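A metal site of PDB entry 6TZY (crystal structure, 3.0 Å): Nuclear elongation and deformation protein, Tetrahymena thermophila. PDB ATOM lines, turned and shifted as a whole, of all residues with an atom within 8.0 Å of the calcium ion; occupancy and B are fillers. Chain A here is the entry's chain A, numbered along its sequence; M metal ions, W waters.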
ATOM      1  N   SER A 145     -12.863 -18.069  23.275  1.00  0.00           N
ATOM      2  CA  SER A 145     -12.155 -17.807  22.031  1.00  0.00           C
ATOM      3  C   SER A 145     -12.846 -16.667  21.290  1.00  0.00           C
ATOM      4  O   SER A 145     -14.066 -16.658  21.153  1.00  0.00           O
ATOM      5  CB  SER A 145     -12.102 -19.057  21.143  1.00  0.00           C
ATOM      6  OG  SER A 145     -11.373 -18.817  19.960  1.00  0.00           O
ATOM      7  N   ASP A 146     -12.060 -15.700  20.824  1.00  0.00           N
ATOM      8  CA  ASP A 146     -12.572 -14.688  19.918  1.00  0.00           C
ATOM      9  C   ASP A 146     -12.665 -15.271  18.506  1.00  0.00           C
ATOM     10  O   ASP A 146     -12.064 -16.309  18.197  1.00  0.00           O
ATOM     11  CB  ASP A 146     -11.679 -13.448  19.918  1.00  0.00           C
ATOM     12  CG  ASP A 146     -12.478 -12.157  19.881  1.00  0.00           C
ATOM     13  OD1 ASP A 146     -13.520 -12.120  19.205  1.00  0.00           O
ATOM     14  OD2 ASP A 146     -12.039 -11.174  20.522  1.00  0.00           O
ATOM     15  N   VAL A 147     -13.444 -14.606  17.660  1.00  0.00           N
ATOM     16  CA  VAL A 147     -13.608 -15.031  16.270  1.00  0.00           C
ATOM     17  C   VAL A 147     -12.773 -14.160  15.349  1.00  0.00           C
ATOM     18  O   VAL A 147     -11.889 -14.651  14.634  1.00  0.00           O
ATOM     19  CB  VAL A 147     -15.091 -14.996  15.845  1.00  0.00           C
ATOM     20  CG1 VAL A 147     -15.230 -15.406  14.393  1.00  0.00           C
ATOM     21  CG2 VAL A 147     -15.925 -15.909  16.739  1.00  0.00           C
ATOM     22  N   ASP A 148     -13.048 -12.855  15.355  1.00  0.00           N
ATOM     23  CA  ASP A 148     -12.359 -11.910  14.495  1.00  0.00           C
ATOM     24  C   ASP A 148     -10.931 -11.704  15.011  1.00  0.00           C
ATOM     25  O   ASP A 148     -10.736 -11.202  16.123  1.00  0.00           O
ATOM     26  CB  ASP A 148     -13.117 -10.594  14.445  1.00  0.00           C
ATOM     27  CG  ASP A 148     -14.478 -10.730  13.797  1.00  0.00           C
ATOM     28  OD1 ASP A 148     -14.596 -11.511  12.827  1.00  0.00           O
ATOM     29  OD2 ASP A 148     -15.424 -10.066  14.265  1.00  0.00           O
ATOM     30  N   GLY A 149      -9.941 -12.093  14.212  1.00  0.00           N
ATOM     31  CA  GLY A 149      -8.555 -11.961  14.572  1.00  0.00           C
ATOM     32  C   GLY A 149      -7.960 -13.196  15.224  1.00  0.00           C
ATOM     33  O   GLY A 149      -6.754 -13.430  15.096  1.00  0.00           O
ATOM     34  N   THR A 150      -8.770 -13.985  15.911  1.00  0.00           N
ATOM     35  CA  THR A 150      -8.325 -15.212  16.560  1.00  0.00           C
ATOM     36  C   THR A 150      -8.626 -16.457  15.744  1.00  0.00           C
ATOM     37  O   THR A 150      -7.778 -17.349  15.655  1.00  0.00           O
ATOM     38  CB  THR A 150      -8.968 -15.337  17.949  1.00  0.00           C
ATOM     39  OG1 THR A 150      -8.900 -14.069  18.618  1.00  0.00           O
ATOM     40  CG2 THR A 150      -8.235 -16.374  18.788  1.00  0.00           C
ATOM     41  N   ASP A 155      -9.086  -8.697  12.064  1.00  0.00           N
ATOM     42  CA  ASP A 155     -10.340  -8.171  12.586  1.00  0.00           C
ATOM     43  C   ASP A 155     -10.488  -6.701  12.223  1.00  0.00           C
ATOM     44  O   ASP A 155     -11.058  -6.369  11.183  1.00  0.00           O
ATOM     45  CB  ASP A 155     -10.409  -8.346  14.110  1.00  0.00           C
ATOM     46  CG  ASP A 155      -9.731  -7.214  14.860  1.00  0.00           C
ATOM     47  OD1 ASP A 155     -10.399  -6.183  15.106  1.00  0.00           O
ATOM     48  OD2 ASP A 155      -8.539  -7.355  15.201  1.00  0.00           O
ATOM     49  N   LEU A 190     -16.802 -15.625  21.005  1.00  0.00           N
ATOM     50  CA  LEU A 190     -17.227 -14.244  21.198  1.00  0.00           C
ATOM     51  C   LEU A 190     -17.114 -13.479  19.885  1.00  0.00           C
ATOM     52  O   LEU A 190     -16.143 -13.652  19.134  1.00  0.00           O
ATOM     53  CB  LEU A 190     -16.378 -13.552  22.267  1.00  0.00           C
ATOM     54  CG  LEU A 190     -16.251 -14.239  23.632  1.00  0.00           C
ATOM     55  CD1 LEU A 190     -15.163 -13.547  24.435  1.00  0.00           C
ATOM     56  CD2 LEU A 190     -17.574 -14.232  24.383  1.00  0.00           C
ATOM     57  N   SER A 192     -18.089  -9.420  18.215  1.00  0.00           N
ATOM     58  CA  SER A 192     -18.602  -8.062  18.281  1.00  0.00           C
ATOM     59  C   SER A 192     -19.064  -7.587  16.902  1.00  0.00           C
ATOM     60  O   SER A 192     -18.929  -6.414  16.550  1.00  0.00           O
ATOM     61  CB  SER A 192     -17.542  -7.112  18.857  1.00  0.00           C
ATOM     62  OG  SER A 192     -16.251  -7.484  18.403  1.00  0.00           O
ATOM     63  N   LYS A 244     -16.589  -5.939  25.318  1.00  0.00           N
ATOM     64  CA  LYS A 244     -16.212  -7.328  25.542  1.00  0.00           C
ATOM     65  C   LYS A 244     -16.002  -7.625  27.016  1.00  0.00           C
ATOM     66  O   LYS A 244     -16.291  -8.734  27.479  1.00  0.00           O
ATOM     67  CB  LYS A 244     -14.950  -7.659  24.746  1.00  0.00           C
ATOM     68  CG  LYS A 244     -14.615  -9.140  24.675  1.00  0.00           C
ATOM     69  CD  LYS A 244     -13.481  -9.394  23.684  1.00  0.00           C
ATOM     70  CE  LYS A 244     -13.876  -9.027  22.254  1.00  0.00           C
ATOM     71  NZ  LYS A 244     -12.710  -9.069  21.326  1.00  0.00           N
ATOM     72  N   PHE A 266      -8.757 -16.980  24.337  1.00  0.00           N
ATOM     73  CA  PHE A 266      -8.009 -16.742  23.117  1.00  0.00           C
ATOM     74  C   PHE A 266      -8.428 -15.403  22.539  1.00  0.00           C
ATOM     75  O   PHE A 266      -9.633 -15.124  22.437  1.00  0.00           O
ATOM     76  CB  PHE A 266      -8.247 -17.868  22.101  1.00  0.00           C
ATOM     77  CG  PHE A 266      -7.620 -19.182  22.487  1.00  0.00           C
ATOM     78  CD1 PHE A 266      -8.258 -20.023  23.386  1.00  0.00           C
ATOM     79  CD2 PHE A 266      -6.396 -19.561  21.970  1.00  0.00           C
ATOM     80  CE1 PHE A 266      -7.683 -21.241  23.747  1.00  0.00           C
ATOM     81  CE2 PHE A 266      -5.821 -20.765  22.328  1.00  0.00           C
ATOM     82  CZ  PHE A 266      -6.470 -21.608  23.218  1.00  0.00           C
ATOM     83  N   GLY A 267      -7.448 -14.581  22.168  1.00  0.00           N
ATOM     84  CA  GLY A 267      -7.731 -13.252  21.672  1.00  0.00           C
ATOM     85  C   GLY A 267      -6.707 -12.816  20.644  1.00  0.00           C
ATOM     86  O   GLY A 267      -5.726 -13.515  20.365  1.00  0.00           O
ATOM     87  N   ASN A 268      -6.946 -11.636  20.076  1.00  0.00           N
ATOM     88  CA  ASN A 268      -6.096 -11.061  19.046  1.00  0.00           C
ATOM     89  C   ASN A 268      -5.453  -9.739  19.438  1.00  0.00           C
ATOM     90  O   ASN A 268      -4.414  -9.385  18.881  1.00  0.00           O
ATOM     91  CB  ASN A 268      -6.888 -10.856  17.748  1.00  0.00           C
ATOM     92  CG  ASN A 268      -7.957  -9.778  17.877  1.00  0.00           C
ATOM     93  OD1 ASN A 268      -8.755  -9.778  18.819  1.00  0.00           O
ATOM     94  ND2 ASN A 268      -7.965  -8.851  16.932  1.00  0.00           N
ATOM     95  N   ARG A 269      -6.038  -8.999  20.375  1.00  0.00           N
ATOM     96  CA  ARG A 269      -5.506  -7.728  20.822  1.00  0.00           C
ATOM     97  C   ARG A 269      -5.200  -7.796  22.316  1.00  0.00           C
ATOM     98  O   ARG A 269      -5.699  -8.667  23.033  1.00  0.00           O
ATOM     99  CB  ARG A 269      -6.482  -6.573  20.528  1.00  0.00           C
ATOM    100  CG  ARG A 269      -6.760  -6.377  19.050  1.00  0.00           C
ATOM    101  CD  ARG A 269      -5.490  -5.991  18.303  1.00  0.00           C
ATOM    102  NE  ARG A 269      -5.765  -5.715  16.886  1.00  0.00           N
ATOM    103  CZ  ARG A 269      -6.077  -4.512  16.411  1.00  0.00           C
ATOM    104  NH1 ARG A 269      -6.168  -3.468  17.231  1.00  0.00           N
ATOM    105  NH2 ARG A 269      -6.314  -4.352  15.117  1.00  0.00           N
ATOM    106  N   ASP A 270      -4.361  -6.866  22.776  1.00  0.00           N
ATOM    107  CA  ASP A 270      -3.989  -6.840  24.181  1.00  0.00           C
ATOM    108  C   ASP A 270      -5.161  -6.482  25.091  1.00  0.00           C
ATOM    109  O   ASP A 270      -5.134  -6.812  26.278  1.00  0.00           O
ATOM    110  CB  ASP A 270      -2.837  -5.863  24.421  1.00  0.00           C
ATOM    111  CG  ASP A 270      -1.500  -6.574  24.577  1.00  0.00           C
ATOM    112  OD1 ASP A 270      -1.509  -7.766  24.942  1.00  0.00           O
ATOM    113  OD2 ASP A 270      -0.455  -5.931  24.340  1.00  0.00           O
ATOM    114  N   THR A 271      -6.192  -5.821  24.553  1.00  0.00           N
ATOM    115  CA  THR A 271      -7.384  -5.551  25.341  1.00  0.00           C
ATOM    116  C   THR A 271      -8.191  -6.827  25.584  1.00  0.00           C
ATOM    117  O   THR A 271      -8.915  -6.923  26.581  1.00  0.00           O
ATOM    118  CB  THR A 271      -8.255  -4.503  24.664  1.00  0.00           C
ATOM    119  OG1 THR A 271      -8.753  -5.027  23.426  1.00  0.00           O
ATOM    120  CG2 THR A 271      -7.453  -3.241  24.394  1.00  0.00           C
ATOM    121  N   ASP A 272      -8.074  -7.811  24.680  1.00  0.00           N
ATOM    122  CA  ASP A 272      -8.668  -9.120  24.941  1.00  0.00           C
ATOM    123  C   ASP A 272      -8.070  -9.743  26.192  1.00  0.00           C
ATOM    124  O   ASP A 272      -8.785 -10.378  26.980  1.00  0.00           O
ATOM    125  CB  ASP A 272      -8.461 -10.038  23.742  1.00  0.00           C
ATOM    126  CG  ASP A 272      -9.221  -9.608  22.504  1.00  0.00           C
ATOM    127  OD1 ASP A 272     -10.076  -8.704  22.610  1.00  0.00           O
ATOM    128  OD2 ASP A 272      -8.956 -10.176  21.431  1.00  0.00           O
ATOM    129  N   ALA A 273      -6.765  -9.564  26.387  1.00  0.00           N
ATOM    130  CA  ALA A 273      -6.102 -10.077  27.584  1.00  0.00           C
ATOM    131  C   ALA A 273      -6.615  -9.371  28.829  1.00  0.00           C
ATOM    132  O   ALA A 273      -6.785 -10.002  29.885  1.00  0.00           O
ATOM    133  CB  ALA A 273      -4.602  -9.898  27.453  1.00  0.00           C
ATOM    134  N   ALA A 275      -9.638  -8.182  29.168  1.00  0.00           N
ATOM    135  CA  ALA A 275     -10.990  -8.665  29.398  1.00  0.00           C
ATOM    136  C   ALA A 275     -10.979 -10.025  30.091  1.00  0.00           C
ATOM    137  O   ALA A 275     -11.859 -10.313  30.924  1.00  0.00           O
ATOM    138  CB  ALA A 275     -11.758  -8.750  28.075  1.00  0.00           C
ATOM    139  N   ILE A 288      -2.648 -14.867  23.128  1.00  0.00           N
ATOM    140  CA  ILE A 288      -2.872 -13.736  22.236  1.00  0.00           C
ATOM    141  C   ILE A 288      -2.121 -13.998  20.936  1.00  0.00           C
ATOM    142  O   ILE A 288      -0.919 -14.303  20.964  1.00  0.00           O
ATOM    143  CB  ILE A 288      -2.421 -12.414  22.866  1.00  0.00           C
ATOM    144  CG1 ILE A 288      -3.280 -12.090  24.093  1.00  0.00           C
ATOM    145  CG2 ILE A 288      -2.491 -11.278  21.848  1.00  0.00           C
ATOM    146  CD1 ILE A 288      -4.714 -11.772  23.752  1.00  0.00           C
HETATM  147 CA    CA M   1     -10.708  -9.213  20.297  1.00  0.00          CA
HETATM  148  O   HOH W   1     -11.356  -9.067  17.887  1.00  0.00           O
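The backbone NH of Arg 269 sits close to the side-chain carboxylate of Asp 272. O of Phe 266 sits at hydrogen-bond distance from N of Asp 146, at 3.0 Å. N of Asn 268 lies within hydrogen-bond range of OG1 of Thr 150 (3.4 Å).
Within 4 Å of the calcium ion: Asp 146, Lys 244, Asn 268 and Asp 272. The nearest printed residue that does not touch the calcium ion is Asp 148 (4.6 Å).
The calcium ion is bound by NZ of Lys 244 (2.3 Å), OD2 of Asp 272 (2.3 Å), OD2 of Asp 146 (2.4 Å), OD1 of Asp 272 (2.5 Å), water W1 (2.5 Å) and OD1 of Asn 268 (2.5 Å). The calcium ion has six donor atoms within binding distance.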
